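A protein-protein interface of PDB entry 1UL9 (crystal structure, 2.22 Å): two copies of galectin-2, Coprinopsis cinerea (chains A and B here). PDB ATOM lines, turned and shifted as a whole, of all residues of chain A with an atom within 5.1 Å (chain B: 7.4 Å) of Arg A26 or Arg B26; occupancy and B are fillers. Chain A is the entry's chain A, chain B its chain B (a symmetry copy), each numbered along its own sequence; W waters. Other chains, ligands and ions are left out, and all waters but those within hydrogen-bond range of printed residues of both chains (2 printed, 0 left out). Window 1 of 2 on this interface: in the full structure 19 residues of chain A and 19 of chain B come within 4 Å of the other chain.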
ATOM      1  N   LEU A   2      -3.965 -24.075  -8.965  1.00  0.00           N
ATOM      2  CA  LEU A   2      -5.199 -23.845  -9.700  1.00  0.00           C
ATOM      3  C   LEU A   2      -5.301 -24.714 -10.946  1.00  0.00           C
ATOM      4  O   LEU A   2      -4.344 -24.824 -11.718  1.00  0.00           O
ATOM      5  CB  LEU A   2      -5.306 -22.373 -10.121  1.00  0.00           C
ATOM      6  CG  LEU A   2      -6.399 -22.088 -11.161  1.00  0.00           C
ATOM      7  CD1 LEU A   2      -7.761 -22.381 -10.556  1.00  0.00           C
ATOM      8  CD2 LEU A   2      -6.324 -20.637 -11.629  1.00  0.00           C
ATOM      9  N   HIS A   4      -8.258 -26.032 -14.189  1.00  0.00           N
ATOM     10  CA  HIS A   4      -9.512 -25.759 -14.878  1.00  0.00           C
ATOM     11  C   HIS A   4      -9.999 -27.112 -15.375  1.00  0.00           C
ATOM     12  O   HIS A   4      -9.516 -27.634 -16.373  1.00  0.00           O
ATOM     13  CB  HIS A   4      -9.289 -24.781 -16.034  1.00  0.00           C
ATOM     14  CG  HIS A   4      -9.183 -23.354 -15.589  1.00  0.00           C
ATOM     15  ND1 HIS A   4      -8.265 -22.472 -16.118  1.00  0.00           N
ATOM     16  CD2 HIS A   4      -9.880 -22.658 -14.659  1.00  0.00           C
ATOM     17  CE1 HIS A   4      -8.400 -21.296 -15.530  1.00  0.00           C
ATOM     18  NE2 HIS A   4      -9.373 -21.383 -14.641  1.00  0.00           N
ATOM     19  N   ALA A  24     -10.865 -27.234  -3.577  1.00  0.00           N
ATOM     20  CA  ALA A  24     -11.946 -26.261  -3.581  1.00  0.00           C
ATOM     21  C   ALA A  24     -12.435 -26.101  -5.015  1.00  0.00           C
ATOM     22  O   ALA A  24     -11.831 -25.380  -5.817  1.00  0.00           O
ATOM     23  CB  ALA A  24     -11.456 -24.922  -3.029  1.00  0.00           C
ATOM     24  N   ILE A  25     -13.521 -26.806  -5.326  1.00  0.00           N
ATOM     25  CA  ILE A  25     -14.128 -26.783  -6.647  1.00  0.00           C
ATOM     26  C   ILE A  25     -15.218 -25.720  -6.679  1.00  0.00           C
ATOM     27  O   ILE A  25     -16.141 -25.742  -5.859  1.00  0.00           O
ATOM     28  CB  ILE A  25     -14.790 -28.138  -6.977  1.00  0.00           C
ATOM     29  CG1 ILE A  25     -13.761 -29.269  -6.865  1.00  0.00           C
ATOM     30  CG2 ILE A  25     -15.408 -28.088  -8.371  1.00  0.00           C
ATOM     31  CD1 ILE A  25     -14.372 -30.654  -6.929  1.00  0.00           C
ATOM     32  N   ARG A  26     -15.121 -24.796  -7.626  1.00  0.00           N
ATOM     33  CA  ARG A  26     -16.128 -23.750  -7.740  1.00  0.00           C
ATOM     34  C   ARG A  26     -16.643 -23.614  -9.166  1.00  0.00           C
ATOM     35  O   ARG A  26     -15.875 -23.691 -10.121  1.00  0.00           O
ATOM     36  CB  ARG A  26     -15.559 -22.415  -7.254  1.00  0.00           C
ATOM     37  CG  ARG A  26     -15.174 -22.426  -5.780  1.00  0.00           C
ATOM     38  CD  ARG A  26     -14.722 -21.050  -5.315  1.00  0.00           C
ATOM     39  NE  ARG A  26     -13.505 -20.610  -5.993  1.00  0.00           N
ATOM     40  CZ  ARG A  26     -13.364 -19.418  -6.562  1.00  0.00           C
ATOM     41  NH1 ARG A  26     -14.365 -18.551  -6.538  1.00  0.00           N
ATOM     42  NH2 ARG A  26     -12.223 -19.094  -7.156  1.00  0.00           N
ATOM     43  N   SER A  27     -17.951 -23.418  -9.297  1.00  0.00           N
ATOM     44  CA  SER A  27     -18.588 -23.266 -10.597  1.00  0.00           C
ATOM     45  C   SER A  27     -18.971 -21.814 -10.854  1.00  0.00           C
ATOM     46  O   SER A  27     -19.366 -21.098  -9.936  1.00  0.00           O
ATOM     47  CB  SER A  27     -19.847 -24.132 -10.670  1.00  0.00           C
ATOM     48  OG  SER A  27     -20.526 -23.918 -11.889  1.00  0.00           O
ATOM     49  N   SER A  28     -18.870 -21.380 -12.106  1.00  0.00           N
ATOM     50  CA  SER A  28     -19.219 -20.002 -12.441  1.00  0.00           C
ATOM     51  C   SER A  28     -20.700 -19.891 -12.783  1.00  0.00           C
ATOM     52  O   SER A  28     -21.170 -18.844 -13.225  1.00  0.00           O
ATOM     53  CB  SER A  28     -18.376 -19.506 -13.614  1.00  0.00           C
ATOM     54  OG  SER A  28     -18.534 -20.335 -14.749  1.00  0.00           O
ATOM     55  N   PRO A  89     -22.200 -22.257  -7.314  1.00  0.00           N
ATOM     56  CA  PRO A  89     -22.199 -23.433  -6.437  1.00  0.00           C
ATOM     57  C   PRO A  89     -20.795 -24.010  -6.281  1.00  0.00           C
ATOM     58  O   PRO A  89     -19.960 -23.861  -7.166  1.00  0.00           O
ATOM     59  CB  PRO A  89     -23.162 -24.387  -7.139  1.00  0.00           C
ATOM     60  CG  PRO A  89     -23.040 -24.000  -8.576  1.00  0.00           C
ATOM     61  CD  PRO A  89     -23.013 -22.498  -8.518  1.00  0.00           C
ATOM     62  N   SER A  90     -20.536 -24.670  -5.158  1.00  0.00           N
ATOM     63  CA  SER A  90     -19.213 -25.236  -4.920  1.00  0.00           C
ATOM     64  C   SER A  90     -19.240 -26.586  -4.223  1.00  0.00           C
ATOM     65  O   SER A  90     -20.253 -26.996  -3.663  1.00  0.00           O
ATOM     66  CB  SER A  90     -18.381 -24.275  -4.069  1.00  0.00           C
ATOM     67  OG  SER A  90     -18.860 -24.241  -2.734  1.00  0.00           O
ATOM     68  N   SER A 133     -20.815 -25.078 -14.539  1.00  0.00           N
ATOM     69  CA  SER A 133     -20.093 -24.534 -15.672  1.00  0.00           C
ATOM     70  C   SER A 133     -18.998 -25.484 -16.120  1.00  0.00           C
ATOM     71  O   SER A 133     -18.611 -26.404 -15.396  1.00  0.00           O
ATOM     72  CB  SER A 133     -19.440 -23.205 -15.289  1.00  0.00           C
ATOM     73  OG  SER A 133     -18.441 -23.419 -14.302  1.00  0.00           O
ATOM     74  N   VAL A 136     -14.821 -25.976 -14.323  1.00  0.00           N
ATOM     75  CA  VAL A 136     -15.087 -25.541 -12.961  1.00  0.00           C
ATOM     76  C   VAL A 136     -13.709 -25.149 -12.448  1.00  0.00           C
ATOM     77  O   VAL A 136     -12.698 -25.721 -12.872  1.00  0.00           O
ATOM     78  CB  VAL A 136     -15.652 -26.667 -12.048  1.00  0.00           C
ATOM     79  CG1 VAL A 136     -17.113 -26.930 -12.380  1.00  0.00           C
ATOM     80  CG2 VAL A 136     -14.827 -27.940 -12.203  1.00  0.00           C
ATOM     81  N   THR A 137     -13.658 -24.155 -11.569  1.00  0.00           N
ATOM     82  CA  THR A 137     -12.389 -23.723 -11.007  1.00  0.00           C
ATOM     83  C   THR A 137     -12.047 -24.688  -9.887  1.00  0.00           C
ATOM     84  O   THR A 137     -12.919 -25.078  -9.105  1.00  0.00           O
ATOM     85  CB  THR A 137     -12.484 -22.289 -10.449  1.00  0.00           C
ATOM     86  OG1 THR A 137     -12.522 -21.360 -11.538  1.00  0.00           O
ATOM     87  CG2 THR A 137     -11.287 -21.971  -9.560  1.00  0.00           C
ATOM     88  N   VAL A 138     -10.787 -25.094  -9.814  1.00  0.00           N
ATOM     89  CA  VAL A 138     -10.375 -26.015  -8.765  1.00  0.00           C
ATOM     90  C   VAL A 138      -9.031 -25.630  -8.166  1.00  0.00           C
ATOM     91  O   VAL A 138      -8.008 -25.654  -8.845  1.00  0.00           O
ATOM     92  CB  VAL A 138     -10.252 -27.466  -9.282  1.00  0.00           C
ATOM     93  CG1 VAL A 138     -10.003 -28.409  -8.112  1.00  0.00           C
ATOM     94  CG2 VAL A 138     -11.507 -27.872 -10.029  1.00  0.00           C
ATOM     95  N   ASP A 139      -9.042 -25.258  -6.893  1.00  0.00           N
ATOM     96  CA  ASP A 139      -7.807 -24.929  -6.203  1.00  0.00           C
ATOM     97  C   ASP A 139      -7.539 -26.101  -5.277  1.00  0.00           C
ATOM     98  O   ASP A 139      -8.388 -26.469  -4.465  1.00  0.00           O
ATOM     99  CB  ASP A 139      -7.947 -23.638  -5.389  1.00  0.00           C
ATOM    100  CG  ASP A 139      -7.938 -22.400  -6.261  1.00  0.00           C
ATOM    101  OD1 ASP A 139      -9.023 -21.886  -6.587  1.00  0.00           O
ATOM    102  OD2 ASP A 139      -6.836 -21.950  -6.634  1.00  0.00           O
ATOM    103  N   MET B   1     -18.069 -12.940  -6.607  1.00  0.00           N
ATOM    104  CA  MET B   1     -18.684 -13.488  -7.843  1.00  0.00           C
ATOM    105  C   MET B   1     -17.603 -14.092  -8.732  1.00  0.00           C
ATOM    106  O   MET B   1     -16.631 -13.422  -9.079  1.00  0.00           O
ATOM    107  CB  MET B   1     -19.413 -12.379  -8.602  1.00  0.00           C
ATOM    108  CG  MET B   1     -20.090 -12.852  -9.879  1.00  0.00           C
ATOM    109  SD  MET B   1     -21.482 -13.960  -9.562  1.00  0.00           S
ATOM    110  CE  MET B   1     -22.855 -12.848  -9.808  1.00  0.00           C
ATOM    111  N   LEU B   2     -17.773 -15.360  -9.094  1.00  0.00           N
ATOM    112  CA  LEU B   2     -16.808 -16.049  -9.945  1.00  0.00           C
ATOM    113  C   LEU B   2     -17.250 -16.087 -11.406  1.00  0.00           C
ATOM    114  O   LEU B   2     -18.392 -16.434 -11.712  1.00  0.00           O
ATOM    115  CB  LEU B   2     -16.593 -17.486  -9.457  1.00  0.00           C
ATOM    116  CG  LEU B   2     -15.831 -18.410 -10.412  1.00  0.00           C
ATOM    117  CD1 LEU B   2     -14.367 -17.982 -10.492  1.00  0.00           C
ATOM    118  CD2 LEU B   2     -15.931 -19.848  -9.918  1.00  0.00           C
ATOM    119  N   TYR B   3     -16.335 -15.722 -12.296  1.00  0.00           N
ATOM    120  CA  TYR B   3     -16.592 -15.741 -13.732  1.00  0.00           C
ATOM    121  C   TYR B   3     -15.473 -16.522 -14.408  1.00  0.00           C
ATOM    122  O   TYR B   3     -14.369 -16.652 -13.867  1.00  0.00           O
ATOM    123  CB  TYR B   3     -16.584 -14.330 -14.341  1.00  0.00           C
ATOM    124  CG  TYR B   3     -17.554 -13.335 -13.748  1.00  0.00           C
ATOM    125  CD1 TYR B   3     -17.186 -12.532 -12.672  1.00  0.00           C
ATOM    126  CD2 TYR B   3     -18.828 -13.164 -14.295  1.00  0.00           C
ATOM    127  CE1 TYR B   3     -18.061 -11.571 -12.152  1.00  0.00           C
ATOM    128  CE2 TYR B   3     -19.712 -12.212 -13.783  1.00  0.00           C
ATOM    129  CZ  TYR B   3     -19.320 -11.417 -12.715  1.00  0.00           C
ATOM    130  OH  TYR B   3     -20.176 -10.452 -12.229  1.00  0.00           O
ATOM    131  N   HIS B   4     -15.763 -17.040 -15.594  1.00  0.00           N
ATOM    132  CA  HIS B   4     -14.772 -17.755 -16.378  1.00  0.00           C
ATOM    133  C   HIS B   4     -14.674 -16.970 -17.675  1.00  0.00           C
ATOM    134  O   HIS B   4     -15.572 -17.009 -18.516  1.00  0.00           O
ATOM    135  CB  HIS B   4     -15.212 -19.199 -16.627  1.00  0.00           C
ATOM    136  CG  HIS B   4     -14.997 -20.102 -15.450  1.00  0.00           C
ATOM    137  ND1 HIS B   4     -15.964 -20.968 -14.984  1.00  0.00           N
ATOM    138  CD2 HIS B   4     -13.923 -20.267 -14.640  1.00  0.00           C
ATOM    139  CE1 HIS B   4     -15.496 -21.623 -13.936  1.00  0.00           C
ATOM    140  NE2 HIS B   4     -14.260 -21.217 -13.706  1.00  0.00           N
ATOM    141  N   ALA B  23     -10.864  -7.212  -8.749  1.00  0.00           N
ATOM    142  CA  ALA B  23     -10.937  -8.305  -9.703  1.00  0.00           C
ATOM    143  C   ALA B  23      -9.642  -9.086  -9.575  1.00  0.00           C
ATOM    144  O   ALA B  23      -8.559  -8.554  -9.823  1.00  0.00           O
ATOM    145  CB  ALA B  23     -11.092  -7.774 -11.124  1.00  0.00           C
ATOM    146  N   ALA B  24      -9.755 -10.342  -9.158  1.00  0.00           N
ATOM    147  CA  ALA B  24      -8.589 -11.197  -9.004  1.00  0.00           C
ATOM    148  C   ALA B  24      -8.599 -12.197 -10.147  1.00  0.00           C
ATOM    149  O   ALA B  24      -9.368 -13.158 -10.131  1.00  0.00           O
ATOM    150  CB  ALA B  24      -8.638 -11.922  -7.660  1.00  0.00           C
ATOM    151  N   ILE B  25      -7.758 -11.948 -11.148  1.00  0.00           N
ATOM    152  CA  ILE B  25      -7.658 -12.815 -12.317  1.00  0.00           C
ATOM    153  C   ILE B  25      -6.533 -13.813 -12.110  1.00  0.00           C
ATOM    154  O   ILE B  25      -5.408 -13.428 -11.795  1.00  0.00           O
ATOM    155  CB  ILE B  25      -7.332 -12.011 -13.591  1.00  0.00           C
ATOM    156  CG1 ILE B  25      -8.409 -10.957 -13.842  1.00  0.00           C
ATOM    157  CG2 ILE B  25      -7.214 -12.957 -14.777  1.00  0.00           C
ATOM    158  CD1 ILE B  25      -8.103 -10.034 -15.002  1.00  0.00           C
ATOM    159  N   ARG B  26      -6.832 -15.092 -12.298  1.00  0.00           N
ATOM    160  CA  ARG B  26      -5.831 -16.132 -12.118  1.00  0.00           C
ATOM    161  C   ARG B  26      -5.822 -17.127 -13.273  1.00  0.00           C
ATOM    162  O   ARG B  26      -6.870 -17.631 -13.690  1.00  0.00           O
ATOM    163  CB  ARG B  26      -6.073 -16.872 -10.801  1.00  0.00           C
ATOM    164  CG  ARG B  26      -5.940 -16.005  -9.566  1.00  0.00           C
ATOM    165  CD  ARG B  26      -6.104 -16.853  -8.311  1.00  0.00           C
ATOM    166  NE  ARG B  26      -7.457 -17.396  -8.189  1.00  0.00           N
ATOM    167  CZ  ARG B  26      -7.729 -18.666  -7.902  1.00  0.00           C
ATOM    168  NH1 ARG B  26      -6.739 -19.532  -7.711  1.00  0.00           N
ATOM    169  NH2 ARG B  26      -8.990 -19.068  -7.792  1.00  0.00           N
ATOM    170  N   SER B  27      -4.627 -17.411 -13.776  1.00  0.00           N
ATOM    171  CA  SER B  27      -4.451 -18.336 -14.882  1.00  0.00           C
ATOM    172  C   SER B  27      -4.038 -19.715 -14.377  1.00  0.00           C
ATOM    173  O   SER B  27      -3.239 -19.832 -13.446  1.00  0.00           O
ATOM    174  CB  SER B  27      -3.382 -17.799 -15.839  1.00  0.00           C
ATOM    175  OG  SER B  27      -3.183 -18.681 -16.929  1.00  0.00           O
ATOM    176  N   SER B  28      -4.579 -20.760 -14.992  1.00  0.00           N
ATOM    177  CA  SER B  28      -4.241 -22.117 -14.584  1.00  0.00           C
ATOM    178  C   SER B  28      -2.911 -22.545 -15.193  1.00  0.00           C
ATOM    179  O   SER B  28      -2.418 -23.637 -14.915  1.00  0.00           O
ATOM    180  CB  SER B  28      -5.345 -23.095 -15.004  1.00  0.00           C
ATOM    181  OG  SER B  28      -5.554 -23.083 -16.407  1.00  0.00           O
ATOM    182  N   ALA B  29      -2.326 -21.681 -16.018  1.00  0.00           N
ATOM    183  CA  ALA B  29      -1.053 -21.999 -16.655  1.00  0.00           C
ATOM    184  C   ALA B  29      -0.331 -20.771 -17.192  1.00  0.00           C
ATOM    185  O   ALA B  29      -0.856 -19.661 -17.171  1.00  0.00           O
ATOM    186  CB  ALA B  29      -1.278 -22.999 -17.790  1.00  0.00           C
ATOM    187  N   PHE B  39      -6.218  -7.509 -21.665  1.00  0.00           N
ATOM    188  CA  PHE B  39      -7.369  -7.526 -20.762  1.00  0.00           C
ATOM    189  C   PHE B  39      -7.945  -6.117 -20.771  1.00  0.00           C
ATOM    190  O   PHE B  39      -7.233  -5.149 -20.508  1.00  0.00           O
ATOM    191  CB  PHE B  39      -6.992  -7.904 -19.324  1.00  0.00           C
ATOM    192  CG  PHE B  39      -6.735  -9.371 -19.132  1.00  0.00           C
ATOM    193  CD1 PHE B  39      -5.437  -9.868 -19.118  1.00  0.00           C
ATOM    194  CD2 PHE B  39      -7.797 -10.263 -18.994  1.00  0.00           C
ATOM    195  CE1 PHE B  39      -5.197 -11.234 -18.968  1.00  0.00           C
ATOM    196  CE2 PHE B  39      -7.570 -11.633 -18.844  1.00  0.00           C
ATOM    197  CZ  PHE B  39      -6.269 -12.118 -18.831  1.00  0.00           C
ATOM    198  N   ASN B  88       0.806 -20.607 -12.256  1.00  0.00           N
ATOM    199  CA  ASN B  88      -0.477 -19.931 -12.089  1.00  0.00           C
ATOM    200  C   ASN B  88      -0.293 -18.419 -11.941  1.00  0.00           C
ATOM    201  O   ASN B  88      -0.541 -17.856 -10.876  1.00  0.00           O
ATOM    202  CB  ASN B  88      -1.200 -20.479 -10.853  1.00  0.00           C
ATOM    203  CG  ASN B  88      -1.604 -21.938 -10.999  1.00  0.00           C
ATOM    204  OD1 ASN B  88      -2.054 -22.555 -10.041  1.00  0.00           O
ATOM    205  ND2 ASN B  88      -1.450 -22.491 -12.199  1.00  0.00           N
ATOM    206  N   PRO B  89       0.145 -17.742 -13.013  1.00  0.00           N
ATOM    207  CA  PRO B  89       0.352 -16.292 -12.962  1.00  0.00           C
ATOM    208  C   PRO B  89      -0.965 -15.580 -12.699  1.00  0.00           C
ATOM    209  O   PRO B  89      -2.029 -16.108 -13.026  1.00  0.00           O
ATOM    210  CB  PRO B  89       0.931 -15.982 -14.339  1.00  0.00           C
ATOM    211  CG  PRO B  89       0.265 -16.994 -15.208  1.00  0.00           C
ATOM    212  CD  PRO B  89       0.348 -18.256 -14.379  1.00  0.00           C
ATOM    213  N   SER B  90      -0.905 -14.387 -12.111  1.00  0.00           N
ATOM    214  CA  SER B  90      -2.130 -13.657 -11.807  1.00  0.00           C
ATOM    215  C   SER B  90      -2.053 -12.140 -11.967  1.00  0.00           C
ATOM    216  O   SER B  90      -0.973 -11.546 -12.004  1.00  0.00           O
ATOM    217  CB  SER B  90      -2.573 -13.961 -10.381  1.00  0.00           C
ATOM    218  OG  SER B  90      -1.735 -13.288  -9.457  1.00  0.00           O
ATOM    219  N   ILE B  91      -3.230 -11.528 -12.044  1.00  0.00           N
ATOM    220  CA  ILE B  91      -3.364 -10.084 -12.176  1.00  0.00           C
ATOM    221  C   ILE B  91      -4.500  -9.659 -11.262  1.00  0.00           C
ATOM    222  O   ILE B  91      -5.580 -10.255 -11.291  1.00  0.00           O
ATOM    223  CB  ILE B  91      -3.744  -9.663 -13.608  1.00  0.00           C
ATOM    224  CG1 ILE B  91      -2.761 -10.266 -14.615  1.00  0.00           C
ATOM    225  CG2 ILE B  91      -3.771  -8.133 -13.702  1.00  0.00           C
ATOM    226  CD1 ILE B  91      -3.086  -9.925 -16.067  1.00  0.00           C
ATOM    227  N   THR B  92      -4.257  -8.635 -10.449  1.00  0.00           N
ATOM    228  CA  THR B  92      -5.274  -8.142  -9.530  1.00  0.00           C
ATOM    229  C   THR B  92      -5.473  -6.654  -9.765  1.00  0.00           C
ATOM    230  O   THR B  92      -4.525  -5.870  -9.692  1.00  0.00           O
ATOM    231  CB  THR B  92      -4.864  -8.391  -8.064  1.00  0.00           C
ATOM    232  OG1 THR B  92      -4.699  -9.800  -7.855  1.00  0.00           O
ATOM    233  CG2 THR B  92      -5.929  -7.868  -7.109  1.00  0.00           C
ATOM    234  N   ASP B 105       2.295 -10.794  -9.984  1.00  0.00           N
ATOM    235  CA  ASP B 105       2.827 -11.724  -8.998  1.00  0.00           C
ATOM    236  C   ASP B 105       4.074 -11.208  -8.291  1.00  0.00           C
ATOM    237  O   ASP B 105       4.320 -11.563  -7.141  1.00  0.00           O
ATOM    238  CB  ASP B 105       3.115 -13.069  -9.661  1.00  0.00           C
ATOM    239  CG  ASP B 105       1.857 -13.739 -10.168  1.00  0.00           C
ATOM    240  OD1 ASP B 105       0.953 -13.991  -9.340  1.00  0.00           O
ATOM    241  OD2 ASP B 105       1.773 -14.005 -11.385  1.00  0.00           O
ATOM    242  N   PHE B 132      -1.663 -16.834 -21.217  1.00  0.00           N
ATOM    243  CA  PHE B 132      -2.385 -17.503 -20.139  1.00  0.00           C
ATOM    244  C   PHE B 132      -3.408 -18.548 -20.583  1.00  0.00           C
ATOM    245  O   PHE B 132      -3.690 -18.710 -21.773  1.00  0.00           O
ATOM    246  CB  PHE B 132      -3.078 -16.444 -19.277  1.00  0.00           C
ATOM    247  CG  PHE B 132      -2.157 -15.346 -18.811  1.00  0.00           C
ATOM    248  CD1 PHE B 132      -2.518 -14.008 -18.957  1.00  0.00           C
ATOM    249  CD2 PHE B 132      -0.936 -15.646 -18.218  1.00  0.00           C
ATOM    250  CE1 PHE B 132      -1.675 -12.985 -18.522  1.00  0.00           C
ATOM    251  CE2 PHE B 132      -0.080 -14.624 -17.774  1.00  0.00           C
ATOM    252  CZ  PHE B 132      -0.455 -13.294 -17.928  1.00  0.00           C
ATOM    253  N   SER B 133      -3.971 -19.249 -19.603  1.00  0.00           N
ATOM    254  CA  SER B 133      -4.961 -20.275 -19.875  1.00  0.00           C
ATOM    255  C   SER B 133      -6.259 -19.659 -20.374  1.00  0.00           C
ATOM    256  O   SER B 133      -6.495 -18.463 -20.228  1.00  0.00           O
ATOM    257  CB  SER B 133      -5.261 -21.076 -18.605  1.00  0.00           C
ATOM    258  OG  SER B 133      -5.966 -20.286 -17.655  1.00  0.00           O
ATOM    259  N   PRO B 135     -10.344 -20.740 -20.160  1.00  0.00           N
ATOM    260  CA  PRO B 135     -10.502 -19.369 -19.666  1.00  0.00           C
ATOM    261  C   PRO B 135      -9.533 -19.060 -18.531  1.00  0.00           C
ATOM    262  O   PRO B 135      -8.622 -19.837 -18.244  1.00  0.00           O
ATOM    263  CB  PRO B 135     -11.935 -19.368 -19.167  1.00  0.00           C
ATOM    264  CG  PRO B 135     -12.012 -20.738 -18.503  1.00  0.00           C
ATOM    265  CD  PRO B 135     -11.353 -21.634 -19.558  1.00  0.00           C
ATOM    266  N   VAL B 136      -9.733 -17.902 -17.907  1.00  0.00           N
ATOM    267  CA  VAL B 136      -8.950 -17.498 -16.750  1.00  0.00           C
ATOM    268  C   VAL B 136      -9.988 -17.402 -15.647  1.00  0.00           C
ATOM    269  O   VAL B 136     -11.143 -17.053 -15.906  1.00  0.00           O
ATOM    270  CB  VAL B 136      -8.279 -16.103 -16.906  1.00  0.00           C
ATOM    271  CG1 VAL B 136      -7.044 -16.206 -17.785  1.00  0.00           C
ATOM    272  CG2 VAL B 136      -9.265 -15.108 -17.490  1.00  0.00           C
ATOM    273  N   THR B 137      -9.597 -17.740 -14.426  1.00  0.00           N
ATOM    274  CA  THR B 137     -10.521 -17.642 -13.313  1.00  0.00           C
ATOM    275  C   THR B 137     -10.536 -16.189 -12.870  1.00  0.00           C
ATOM    276  O   THR B 137      -9.480 -15.585 -12.695  1.00  0.00           O
ATOM    277  CB  THR B 137     -10.087 -18.526 -12.137  1.00  0.00           C
ATOM    278  OG1 THR B 137     -10.432 -19.884 -12.416  1.00  0.00           O
ATOM    279  CG2 THR B 137     -10.783 -18.091 -10.850  1.00  0.00           C
ATOM    280  N   VAL B 138     -11.729 -15.627 -12.712  1.00  0.00           N
ATOM    281  CA  VAL B 138     -11.850 -14.245 -12.274  1.00  0.00           C
ATOM    282  C   VAL B 138     -12.856 -14.100 -11.139  1.00  0.00           C
ATOM    283  O   VAL B 138     -14.038 -14.408 -11.306  1.00  0.00           O
ATOM    284  CB  VAL B 138     -12.308 -13.307 -13.415  1.00  0.00           C
ATOM    285  CG1 VAL B 138     -12.173 -11.854 -12.960  1.00  0.00           C
ATOM    286  CG2 VAL B 138     -11.490 -13.555 -14.689  1.00  0.00           C
ATOM    287  N   ASP B 139     -12.375 -13.638  -9.987  1.00  0.00           N
ATOM    288  CA  ASP B 139     -13.221 -13.393  -8.822  1.00  0.00           C
ATOM    289  C   ASP B 139     -13.339 -11.880  -8.645  1.00  0.00           C
ATOM    290  O   ASP B 139     -12.338 -11.190  -8.436  1.00  0.00           O
ATOM    291  CB  ASP B 139     -12.615 -14.008  -7.560  1.00  0.00           C
ATOM    292  CG  ASP B 139     -12.865 -15.496  -7.462  1.00  0.00           C
ATOM    293  OD1 ASP B 139     -11.952 -16.278  -7.791  1.00  0.00           O
ATOM    294  OD2 ASP B 139     -13.986 -15.879  -7.062  1.00  0.00           O
HETATM  295  O   HOH W   1      -3.218 -25.971 -13.875  1.00  0.00           O
HETATM  296  O   HOH W   2     -20.489 -16.440 -13.285  1.00  0.00           O
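N of Leu A2 lies within hydrogen-bond range of OD1 of Asn B88 (2.7 Å).
A ring nitrogen (ND1) of His A4 is in hydrogen-bond range of the side-chain hydroxyl (OG) of Ser B28, 2.8 Å away.
The backbone carbonyl oxygen (O) of Pro B135 sits close to a ring nitrogen (ND1) of His A4, 3.4 Å away.
NE2 of His A4 sits at hydrogen-bond distance from OG1 of Thr B137, 2.9 Å away.
NH1 of Arg A26 lies within salt-bridge range of OD2 of Asp B139 (2.7 Å).
The side-chain hydroxyl (OG) of Ser A28 is in hydrogen-bond range of a ring nitrogen (ND1) of His B4 (2.7 Å).
The side-chain hydroxyl (OG1) of Thr A137 lies within hydrogen-bond range of a ring nitrogen (NE2) of His B4, at 2.8 Å.
The side-chain hydroxyl (OG1) of Thr A137 lies within hydrogen-bond range of the side-chain hydroxyl (OG1) of Thr B137 (2.7 Å).
The side-chain carboxylate (OD2) of Asp A139 lies within salt-bridge range of the guanidinium group (NH1) of Arg B26.
NH2 of Arg A26 lies close to NH2 of Arg B26 (3.3 Å).
N of Ser A27 is in hydrogen-bond range of O of Pro A89, 3.0 Å away.
The backbone NH (N) of Ser A133 sits at hydrogen-bond distance from the side-chain hydroxyl (OG) of Ser A27 (2.9 Å).
N of Ser A28 sits at hydrogen-bond distance from OG of Ser A133 (3.0 Å).
OG of Ser B27 is in hydrogen-bond range of O of Ala B29, at 2.5 Å.
O of Ser B28 is in hydrogen-bond range of ND2 of Asn B88, 3.1 Å away.
The backbone NH (N) of Ser B28 is in hydrogen-bond range of the side-chain hydroxyl (OG) of Ser B133, at 3.0 Å.
Leu A2 touches Arg B26.
Ser B27 touches Leu A2 (O to CD2, 3.7 Å).
N of Ser B28 touches CD2 of Leu A2, 3.8 Å away.
Ser B133 touches His A4.
CD2 of Leu B2 touches CB of Arg A26, 3.7 Å away.
Leu B2 touches Ser A27 (CD2 to O, 3.7 Å).
CB of Ser A28 touches O of Leu B2 (3.6 Å).
Ser A133 touches His B4 (OG to CE1, 3.5 Å).
CD1 of Leu B2 touches OG1 of Thr A137, at 3.99 Å.
Of the printed residues of chain B, His A4 touches Ser B28 (2.8 Å), Ser B133 (3.4 Å), Pro B135 (3.1 Å) and Thr B137 (2.9 Å).
Of chain B, only Leu B2, Arg B26 and Asp B139 come within 4 Å of Arg A26.
Printed residues of chain A within 4 Å of Leu B2: Arg A26 (3.7 Å), Ser A27 (3.7 Å), Ser A28 (3.6 Å) and Thr A137 (3.99 Å).
Of chain A, only Leu A2 (3.7 Å), Arg A26 (3.3 Å) and Asp A139 (2.6 Å) come within 4 Å of Arg B26.
Of the printed residues of chain A, Pro B135 touches His A4.
The nearest residue of chain A that does not touch Arg B26 is Thr A137 (4.1 Å).
Printed residues of chain B that touch a printed residue of chain A: Leu B2, His B4, Arg B26, Ser B27, Ser B28, Asn B88, Ser B133, Pro B135, Thr B137 and Asp B139.
Hydrophobic or aromatic side chains of chain A within 4 Å of the printed part of chain B: Leu A2 and His A4.
Among the printed residues, 19 pairs touch across the chains.
Among the printed residues, Asp or Glu carboxylates within 4 Å of a Lys or Arg side-chain nitrogen of the other chain: Arg A26 with Asp B139 and Asp A139 with Arg B26.
Leu A2 touches Ser B27, and with the chains exchanged Ser A27 touches Leu B2.
His A4 touches Ser B133, and with the chains exchanged Ser A133 touches His B4.
Arg A26 touches Asp B139, and with the chains exchanged Asp A139 touches Arg B26.
Thr A137 touches its own counterpart, Thr B137.
Of the 19 pairs that touch across the chains among the printed residues, 16 have their exchanged pair printed and touching as well.
Water W2 lies within hydrogen-bond range of O of Ser A28 (2.5 Å) and O of Leu B2 (2.6 Å).
Water W1 lies within hydrogen-bond range of O of Ser B28 and O of Leu A2.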
